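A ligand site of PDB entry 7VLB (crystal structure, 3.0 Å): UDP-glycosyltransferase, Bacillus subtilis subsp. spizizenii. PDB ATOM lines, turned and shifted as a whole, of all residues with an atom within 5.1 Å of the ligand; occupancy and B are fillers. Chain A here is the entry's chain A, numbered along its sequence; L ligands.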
ATOM      1  N   TYR A  14     -18.643   5.653 -12.508  1.00  0.00           N
ATOM      2  CA  TYR A  14     -17.657   6.694 -12.871  1.00  0.00           C
ATOM      3  C   TYR A  14     -17.047   6.365 -14.227  1.00  0.00           C
ATOM      4  O   TYR A  14     -16.819   7.257 -15.069  1.00  0.00           O
ATOM      5  CB  TYR A  14     -16.554   6.776 -11.806  1.00  0.00           C
ATOM      6  CG  TYR A  14     -16.983   7.557 -10.594  1.00  0.00           C
ATOM      7  CD1 TYR A  14     -17.003   8.935 -10.622  1.00  0.00           C
ATOM      8  CD2 TYR A  14     -17.420   6.909  -9.449  1.00  0.00           C
ATOM      9  CE1 TYR A  14     -17.414   9.680  -9.527  1.00  0.00           C
ATOM     10  CE2 TYR A  14     -17.846   7.642  -8.349  1.00  0.00           C
ATOM     11  CZ  TYR A  14     -17.847   9.024  -8.387  1.00  0.00           C
ATOM     12  OH  TYR A  14     -18.229   9.762  -7.300  1.00  0.00           O
ATOM     13  N   GLY A  15     -16.739   5.090 -14.439  1.00  0.00           N
ATOM     14  CA  GLY A  15     -16.063   4.699 -15.688  1.00  0.00           C
ATOM     15  C   GLY A  15     -16.953   4.792 -16.888  1.00  0.00           C
ATOM     16  O   GLY A  15     -16.428   4.860 -18.003  1.00  0.00           O
ATOM     17  N   HIS A  16     -18.269   4.774 -16.675  1.00  0.00           N
ATOM     18  CA  HIS A  16     -19.219   4.785 -17.810  1.00  0.00           C
ATOM     19  C   HIS A  16     -19.791   6.192 -17.965  1.00  0.00           C
ATOM     20  O   HIS A  16     -20.476   6.443 -18.948  1.00  0.00           O
ATOM     21  CB  HIS A  16     -20.265   3.685 -17.624  1.00  0.00           C
ATOM     22  CG  HIS A  16     -19.694   2.313 -17.427  1.00  0.00           C
ATOM     23  ND1 HIS A  16     -20.046   1.244 -18.228  1.00  0.00           N
ATOM     24  CD2 HIS A  16     -18.816   1.822 -16.533  1.00  0.00           C
ATOM     25  CE1 HIS A  16     -19.412   0.161 -17.830  1.00  0.00           C
ATOM     26  NE2 HIS A  16     -18.646   0.487 -16.797  1.00  0.00           N
ATOM     27  N   ASN A  18     -17.779   9.204 -16.840  1.00  0.00           N
ATOM     28  CA  ASN A  18     -16.823  10.360 -16.805  1.00  0.00           C
ATOM     29  C   ASN A  18     -16.510  10.901 -18.197  1.00  0.00           C
ATOM     30  O   ASN A  18     -16.410  12.118 -18.359  1.00  0.00           O
ATOM     31  CB  ASN A  18     -15.482  10.033 -16.147  1.00  0.00           C
ATOM     32  CG  ASN A  18     -15.470  10.120 -14.624  1.00  0.00           C
ATOM     33  OD1 ASN A  18     -16.451  10.495 -13.985  1.00  0.00           O
ATOM     34  ND2 ASN A  18     -14.330   9.768 -14.052  1.00  0.00           N
ATOM     35  N   ARG A 207     -13.212  17.853 -13.532  1.00  0.00           N
ATOM     36  CA  ARG A 207     -13.684  16.807 -12.603  1.00  0.00           C
ATOM     37  C   ARG A 207     -13.985  17.488 -11.263  1.00  0.00           C
ATOM     38  O   ARG A 207     -13.277  18.472 -10.943  1.00  0.00           O
ATOM     39  CB  ARG A 207     -12.618  15.707 -12.476  1.00  0.00           C
ATOM     40  CG  ARG A 207     -12.180  15.078 -13.790  1.00  0.00           C
ATOM     41  CD  ARG A 207     -13.166  14.059 -14.342  1.00  0.00           C
ATOM     42  NE  ARG A 207     -12.531  13.089 -15.223  1.00  0.00           N
ATOM     43  CZ  ARG A 207     -11.691  12.136 -14.838  1.00  0.00           C
ATOM     44  NH1 ARG A 207     -11.364  12.012 -13.570  1.00  0.00           N
ATOM     45  NH2 ARG A 207     -11.166  11.323 -15.732  1.00  0.00           N
ATOM     46  N   SER A 226      -4.261   2.594  -8.046  1.00  0.00           N
ATOM     47  CA  SER A 226      -5.734   2.658  -7.974  1.00  0.00           C
ATOM     48  C   SER A 226      -6.336   1.455  -8.700  1.00  0.00           C
ATOM     49  O   SER A 226      -5.816   1.120  -9.774  1.00  0.00           O
ATOM     50  CB  SER A 226      -6.232   3.960  -8.527  1.00  0.00           C
ATOM     51  OG  SER A 226      -7.515   3.808  -9.128  1.00  0.00           O
ATOM     52  N   LEU A 227      -7.363   0.818  -8.146  1.00  0.00           N
ATOM     53  CA  LEU A 227      -8.121  -0.242  -8.861  1.00  0.00           C
ATOM     54  C   LEU A 227      -9.466   0.330  -9.307  1.00  0.00           C
ATOM     55  O   LEU A 227     -10.390  -0.445  -9.601  1.00  0.00           O
ATOM     56  CB  LEU A 227      -8.264  -1.478  -7.959  1.00  0.00           C
ATOM     57  CG  LEU A 227      -6.945  -2.039  -7.403  1.00  0.00           C
ATOM     58  CD1 LEU A 227      -7.191  -3.297  -6.596  1.00  0.00           C
ATOM     59  CD2 LEU A 227      -5.953  -2.346  -8.512  1.00  0.00           C
ATOM     60  N   GLY A 228      -9.545   1.655  -9.447  1.00  0.00           N
ATOM     61  CA  GLY A 228     -10.712   2.324 -10.040  1.00  0.00           C
ATOM     62  C   GLY A 228     -11.745   2.675  -8.998  1.00  0.00           C
ATOM     63  O   GLY A 228     -11.347   3.119  -7.906  1.00  0.00           O
ATOM     64  N   THR A 229     -13.030   2.490  -9.309  1.00  0.00           N
ATOM     65  CA  THR A 229     -14.163   3.018  -8.493  1.00  0.00           C
ATOM     66  C   THR A 229     -15.212   1.946  -8.204  1.00  0.00           C
ATOM     67  O   THR A 229     -16.255   2.316  -7.654  1.00  0.00           O
ATOM     68  CB  THR A 229     -14.778   4.230  -9.187  1.00  0.00           C
ATOM     69  OG1 THR A 229     -15.470   3.770 -10.351  1.00  0.00           O
ATOM     70  CG2 THR A 229     -13.736   5.259  -9.565  1.00  0.00           C
ATOM     71  N   ALA A 230     -14.970   0.675  -8.537  1.00  0.00           N
ATOM     72  CA  ALA A 230     -15.981  -0.406  -8.441  1.00  0.00           C
ATOM     73  C   ALA A 230     -15.353  -1.712  -7.936  1.00  0.00           C
ATOM     74  O   ALA A 230     -15.959  -2.337  -7.076  1.00  0.00           O
ATOM     75  CB  ALA A 230     -16.641  -0.589  -9.783  1.00  0.00           C
ATOM     76  N   PHE A 231     -14.212  -2.138  -8.472  1.00  0.00           N
ATOM     77  CA  PHE A 231     -13.535  -3.381  -8.033  1.00  0.00           C
ATOM     78  C   PHE A 231     -12.263  -3.026  -7.260  1.00  0.00           C
ATOM     79  O   PHE A 231     -11.174  -3.574  -7.550  1.00  0.00           O
ATOM     80  CB  PHE A 231     -13.312  -4.268  -9.248  1.00  0.00           C
ATOM     81  CG  PHE A 231     -14.540  -4.372 -10.103  1.00  0.00           C
ATOM     82  CD1 PHE A 231     -15.491  -5.355  -9.863  1.00  0.00           C
ATOM     83  CD2 PHE A 231     -14.775  -3.451 -11.118  1.00  0.00           C
ATOM     84  CE1 PHE A 231     -16.631  -5.444 -10.642  1.00  0.00           C
ATOM     85  CE2 PHE A 231     -15.918  -3.532 -11.891  1.00  0.00           C
ATOM     86  CZ  PHE A 231     -16.849  -4.527 -11.657  1.00  0.00           C
ATOM     87  N   SER A 255      -4.895   5.311  -4.310  1.00  0.00           N
ATOM     88  CA  SER A 255      -6.348   5.460  -4.088  1.00  0.00           C
ATOM     89  C   SER A 255      -6.901   4.089  -3.678  1.00  0.00           C
ATOM     90  O   SER A 255      -6.656   3.104  -4.432  1.00  0.00           O
ATOM     91  CB  SER A 255      -7.037   6.050  -5.299  1.00  0.00           C
ATOM     92  OG  SER A 255      -8.318   5.469  -5.520  1.00  0.00           O
ATOM     93  N   GLN A 276      -8.856   7.742  -0.206  1.00  0.00           N
ATOM     94  CA  GLN A 276      -9.988   6.984  -0.803  1.00  0.00           C
ATOM     95  C   GLN A 276     -10.099   7.333  -2.287  1.00  0.00           C
ATOM     96  O   GLN A 276     -10.500   6.463  -3.095  1.00  0.00           O
ATOM     97  CB  GLN A 276     -11.289   7.332  -0.098  1.00  0.00           C
ATOM     98  CG  GLN A 276     -11.262   7.081   1.395  1.00  0.00           C
ATOM     99  CD  GLN A 276     -12.676   6.992   1.917  1.00  0.00           C
ATOM    100  OE1 GLN A 276     -13.391   7.993   1.978  1.00  0.00           O
ATOM    101  NE2 GLN A 276     -13.090   5.786   2.260  1.00  0.00           N
ATOM    102  N   SER A 277      -9.751   8.579  -2.620  1.00  0.00           N
ATOM    103  CA  SER A 277      -9.969   9.217  -3.947  1.00  0.00           C
ATOM    104  C   SER A 277      -8.907  10.289  -4.193  1.00  0.00           C
ATOM    105  O   SER A 277      -8.641  11.105  -3.245  1.00  0.00           O
ATOM    106  CB  SER A 277     -11.370   9.774  -4.022  1.00  0.00           C
ATOM    107  OG  SER A 277     -11.524  10.584  -5.175  1.00  0.00           O
ATOM    108  N   VAL A 278      -8.327  10.302  -5.392  1.00  0.00           N
ATOM    109  CA  VAL A 278      -7.305  11.307  -5.807  1.00  0.00           C
ATOM    110  C   VAL A 278      -7.769  11.983  -7.086  1.00  0.00           C
ATOM    111  O   VAL A 278      -8.635  11.454  -7.764  1.00  0.00           O
ATOM    112  CB  VAL A 278      -5.947  10.628  -6.010  1.00  0.00           C
ATOM    113  CG1 VAL A 278      -5.524   9.894  -4.756  1.00  0.00           C
ATOM    114  CG2 VAL A 278      -5.958   9.684  -7.203  1.00  0.00           C
ATOM    115  N   PRO A 279      -7.190  13.157  -7.434  1.00  0.00           N
ATOM    116  CA  PRO A 279      -7.410  13.768  -8.746  1.00  0.00           C
ATOM    117  C   PRO A 279      -6.506  13.103  -9.805  1.00  0.00           C
ATOM    118  O   PRO A 279      -5.393  13.574 -10.069  1.00  0.00           O
ATOM    119  CB  PRO A 279      -7.106  15.238  -8.460  1.00  0.00           C
ATOM    120  CG  PRO A 279      -6.009  15.178  -7.428  1.00  0.00           C
ATOM    121  CD  PRO A 279      -6.294  13.948  -6.596  1.00  0.00           C
ATOM    122  N   GLN A 280      -6.987  11.997 -10.363  1.00  0.00           N
ATOM    123  CA  GLN A 280      -6.194  11.053 -11.170  1.00  0.00           C
ATOM    124  C   GLN A 280      -5.534  11.806 -12.336  1.00  0.00           C
ATOM    125  O   GLN A 280      -4.352  11.512 -12.626  1.00  0.00           O
ATOM    126  CB  GLN A 280      -7.062   9.857 -11.608  1.00  0.00           C
ATOM    127  CG  GLN A 280      -6.249   8.626 -11.960  1.00  0.00           C
ATOM    128  CD  GLN A 280      -7.066   7.418 -12.347  1.00  0.00           C
ATOM    129  OE1 GLN A 280      -7.494   6.622 -11.499  1.00  0.00           O
ATOM    130  NE2 GLN A 280      -7.237   7.255 -13.650  1.00  0.00           N
ATOM    131  N   LEU A 281      -6.227  12.754 -12.970  1.00  0.00           N
ATOM    132  CA  LEU A 281      -5.704  13.493 -14.157  1.00  0.00           C
ATOM    133  C   LEU A 281      -4.508  14.352 -13.734  1.00  0.00           C
ATOM    134  O   LEU A 281      -3.506  14.438 -14.514  1.00  0.00           O
ATOM    135  CB  LEU A 281      -6.806  14.360 -14.768  1.00  0.00           C
ATOM    136  CG  LEU A 281      -8.019  13.611 -15.309  1.00  0.00           C
ATOM    137  CD1 LEU A 281      -8.791  14.482 -16.268  1.00  0.00           C
ATOM    138  CD2 LEU A 281      -7.649  12.290 -15.985  1.00  0.00           C
ATOM    139  N   HIS A 293      -5.864  -1.171 -12.912  1.00  0.00           N
ATOM    140  CA  HIS A 293      -6.675  -2.401 -13.035  1.00  0.00           C
ATOM    141  C   HIS A 293      -7.109  -2.617 -14.484  1.00  0.00           C
ATOM    142  O   HIS A 293      -7.756  -3.636 -14.734  1.00  0.00           O
ATOM    143  CB  HIS A 293      -7.883  -2.294 -12.115  1.00  0.00           C
ATOM    144  CG  HIS A 293      -8.879  -1.275 -12.550  1.00  0.00           C
ATOM    145  ND1 HIS A 293      -8.566   0.070 -12.628  1.00  0.00           N
ATOM    146  CD2 HIS A 293     -10.171  -1.381 -12.897  1.00  0.00           C
ATOM    147  CE1 HIS A 293      -9.631   0.735 -13.022  1.00  0.00           C
ATOM    148  NE2 HIS A 293     -10.627  -0.128 -13.181  1.00  0.00           N
ATOM    149  N   GLY A 295      -9.106  -0.553 -16.275  1.00  0.00           N
ATOM    150  CA  GLY A 295     -10.263   0.268 -16.669  1.00  0.00           C
ATOM    151  C   GLY A 295      -9.936   1.077 -17.902  1.00  0.00           C
ATOM    152  O   GLY A 295      -8.843   1.618 -17.970  1.00  0.00           O
ATOM    153  N   MET A 296     -10.874   1.203 -18.841  1.00  0.00           N
ATOM    154  CA  MET A 296     -10.621   1.927 -20.103  1.00  0.00           C
ATOM    155  C   MET A 296     -10.257   3.374 -19.801  1.00  0.00           C
ATOM    156  O   MET A 296      -9.323   3.880 -20.391  1.00  0.00           O
ATOM    157  CB  MET A 296     -11.805   1.894 -21.056  1.00  0.00           C
ATOM    158  CG  MET A 296     -11.461   2.417 -22.438  1.00  0.00           C
ATOM    159  SD  MET A 296     -10.010   1.660 -23.203  1.00  0.00           S
ATOM    160  CE  MET A 296     -10.618   0.020 -23.598  1.00  0.00           C
ATOM    161  N   ASN A 297     -10.962   4.024 -18.888  1.00  0.00           N
ATOM    162  CA  ASN A 297     -10.641   5.449 -18.569  1.00  0.00           C
ATOM    163  C   ASN A 297      -9.184   5.538 -18.107  1.00  0.00           C
ATOM    164  O   ASN A 297      -8.421   6.361 -18.638  1.00  0.00           O
ATOM    165  CB  ASN A 297     -11.619   6.026 -17.552  1.00  0.00           C
ATOM    166  CG  ASN A 297     -12.979   6.248 -18.193  1.00  0.00           C
ATOM    167  OD1 ASN A 297     -13.213   7.281 -18.804  1.00  0.00           O
ATOM    168  ND2 ASN A 297     -13.837   5.257 -18.092  1.00  0.00           N
ATOM    169  N   SER A 298      -8.830   4.718 -17.124  1.00  0.00           N
ATOM    170  CA  SER A 298      -7.476   4.722 -16.532  1.00  0.00           C
ATOM    171  C   SER A 298      -6.469   4.427 -17.647  1.00  0.00           C
ATOM    172  O   SER A 298      -5.544   5.217 -17.815  1.00  0.00           O
ATOM    173  CB  SER A 298      -7.407   3.748 -15.385  1.00  0.00           C
ATOM    174  OG  SER A 298      -8.323   4.108 -14.363  1.00  0.00           O
ATOM    175  N   GLU A 301      -6.363   7.444 -19.870  1.00  0.00           N
ATOM    176  CA  GLU A 301      -5.873   8.635 -19.116  1.00  0.00           C
ATOM    177  C   GLU A 301      -4.354   8.515 -18.924  1.00  0.00           C
ATOM    178  O   GLU A 301      -3.660   9.559 -18.922  1.00  0.00           O
ATOM    179  CB  GLU A 301      -6.601   8.770 -17.782  1.00  0.00           C
ATOM    180  CG  GLU A 301      -7.990   9.369 -17.922  1.00  0.00           C
ATOM    181  CD  GLU A 301      -8.964   8.922 -16.851  1.00  0.00           C
ATOM    182  OE1 GLU A 301      -8.509   8.662 -15.712  1.00  0.00           O
ATOM    183  OE2 GLU A 301     -10.163   8.805 -17.174  1.00  0.00           O
ATOM    184  N   GLN A 318     -11.556  -6.086 -18.239  1.00  0.00           N
ATOM    185  CA  GLN A 318     -10.285  -5.463 -17.778  1.00  0.00           C
ATOM    186  C   GLN A 318      -9.098  -6.325 -18.232  1.00  0.00           C
ATOM    187  O   GLN A 318      -8.053  -5.736 -18.590  1.00  0.00           O
ATOM    188  CB  GLN A 318     -10.335  -5.280 -16.262  1.00  0.00           C
ATOM    189  CG  GLN A 318     -11.289  -4.178 -15.802  1.00  0.00           C
ATOM    190  CD  GLN A 318     -11.567  -4.236 -14.321  1.00  0.00           C
ATOM    191  OE1 GLN A 318     -10.948  -4.992 -13.580  1.00  0.00           O
ATOM    192  NE2 GLN A 318     -12.510  -3.424 -13.868  1.00  0.00           N
HETATM  193  N1  LIG L   1     -10.843   8.087 -10.704  1.00  0.00           N
HETATM  194  C1  LIG L   1     -10.348   9.257 -10.114  1.00  0.00           C
HETATM  195  N2  LIG L   1      -9.724   9.222  -8.921  1.00  0.00           N
HETATM  196  C2  LIG L   1      -9.545   8.062  -8.254  1.00  0.00           C
HETATM  197  C3  LIG L   1     -10.018   6.884  -8.836  1.00  0.00           C
HETATM  198  C4  LIG L   1     -10.670   6.927 -10.058  1.00  0.00           C
HETATM  199  O1  LIG L   1     -10.520  10.321 -10.740  1.00  0.00           O
HETATM  200  O2  LIG L   1      -8.955   7.994  -7.130  1.00  0.00           O
HETATM  201  C5  LIG L   1     -11.516   8.162 -12.000  1.00  0.00           C
HETATM  202  C6  LIG L   1     -10.501   8.036 -13.133  1.00  0.00           C
HETATM  203  O3  LIG L   1      -9.960   9.306 -13.579  1.00  0.00           O
HETATM  204  C7  LIG L   1     -11.283   7.350 -14.225  1.00  0.00           C
HETATM  205  C8  LIG L   1     -12.397   6.581 -13.522  1.00  0.00           C
HETATM  206  O4  LIG L   1     -12.447   7.072 -12.174  1.00  0.00           O
HETATM  207  O5  LIG L   1     -11.856   8.344 -15.068  1.00  0.00           O
HETATM  208  C9  LIG L   1     -12.125   5.098 -13.525  1.00  0.00           C
HETATM  209  O6  LIG L   1     -12.691   4.535 -14.701  1.00  0.00           O
HETATM  210  P1  LIG L   1     -12.115   3.135 -15.190  1.00  0.00           P
HETATM  211  O7  LIG L   1     -10.617   3.294 -15.179  1.00  0.00           O
HETATM  212  O8  LIG L   1     -12.819   2.676 -16.434  1.00  0.00           O
HETATM  213  O9  LIG L   1     -12.342   2.014 -14.069  1.00  0.00           O
HETATM  214  P2  LIG L   1     -13.709   1.772 -13.264  1.00  0.00           P
HETATM  215  O10 LIG L   1     -13.631   0.333 -12.693  1.00  0.00           O
HETATM  216  O11 LIG L   1     -13.691   2.866 -12.226  1.00  0.00           O
HETATM  217  O12 LIG L   1     -14.795   1.951 -14.301  1.00  0.00           O
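N of Asn 297 lies within hydrogen-bond range of O8 of the ligand, 3.4 Å away. The backbone NH of Met 296 lies within hydrogen-bond range of an oxygen (O8) of the ligand (3.4 Å). An oxygen (O11) of the ligand sits at hydrogen-bond distance from the backbone NH (N) of Thr 229. The side-chain hydroxyl (OG1) of Thr 229 lies within hydrogen-bond range of an oxygen (O11) of the ligand. O5 of the ligand is in hydrogen-bond range of ND2 of Asn 18 (3.0 Å). The side-chain hydroxyl (OG) of Ser 255 is in hydrogen-bond range of an oxygen (O2) of the ligand, at 3.1 Å. A nitrogen (N2) of the ligand sits at hydrogen-bond distance from the backbone carbonyl oxygen of Val 278, 2.7 Å away. The backbone NH of Val 278 is in hydrogen-bond range of an oxygen (O2) of the ligand (3.0 Å). The backbone NH (N) of Ser 298 lies within hydrogen-bond range of an oxygen (O7) of the ligand (3.0 Å). An oxygen (O8) of the ligand is in hydrogen-bond range of the side-chain amide nitrogen of Asn 297 (3.2 Å). An oxygen (O3) of the ligand lies within hydrogen-bond range of the guanidinium group (NH1) of Arg 207, 3.0 Å away. An oxygen (O3) of the ligand sits close to the side-chain amide nitrogen (NE2) of Gln 280 (3.4 Å). O3 of the ligand is in hydrogen-bond range of OE1 of Glu 301 (2.7 Å). An oxygen (O9) of the ligand sits at hydrogen-bond distance from a ring nitrogen (NE2) of His 293, at 2.9 Å. The side-chain hydroxyl (OG) of Ser 298 is in hydrogen-bond range of an oxygen (O7) of the ligand (2.6 Å).
The backbone carbonyl oxygen (O) of Gln 276 lies within hydrogen-bond range of the side-chain hydroxyl (OG) of Ser 255 (3.4 Å). The side-chain amide oxygen (OD1) of Asn 18 sits close to the backbone carbonyl oxygen (O) of Tyr 14, at 3.4 Å. The backbone NH (N) of Gly 295 sits close to a ring nitrogen (NE2) of His 293, at 3.5 Å. OG of Ser 226 sits at hydrogen-bond distance from N of Gly 228 (3.0 Å). The side-chain carboxylate of Glu 301 lies within hydrogen-bond range of the side-chain amide nitrogen of Gln 280 (2.8 Å). The side-chain amide nitrogen (ND2) of Asn 297 is in hydrogen-bond range of the backbone carbonyl oxygen (O) of Gly 15 (2.6 Å). NE2 of Gln 280 lies within hydrogen-bond range of OG of Ser 298. OE2 of Glu 301 lies within salt-bridge range of NH2 of Arg 207 (3.1 Å).
Merely in contact with the ligand: Gly 15, Gly 295, Ser 277, Gly 228 and Ser 226. Hydrophobic or aromatic side chains within 4 Å of the ligand: Val 278 and His 293. The nearest printed residue that does not touch the ligand is Gln 318 (4.1 Å).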
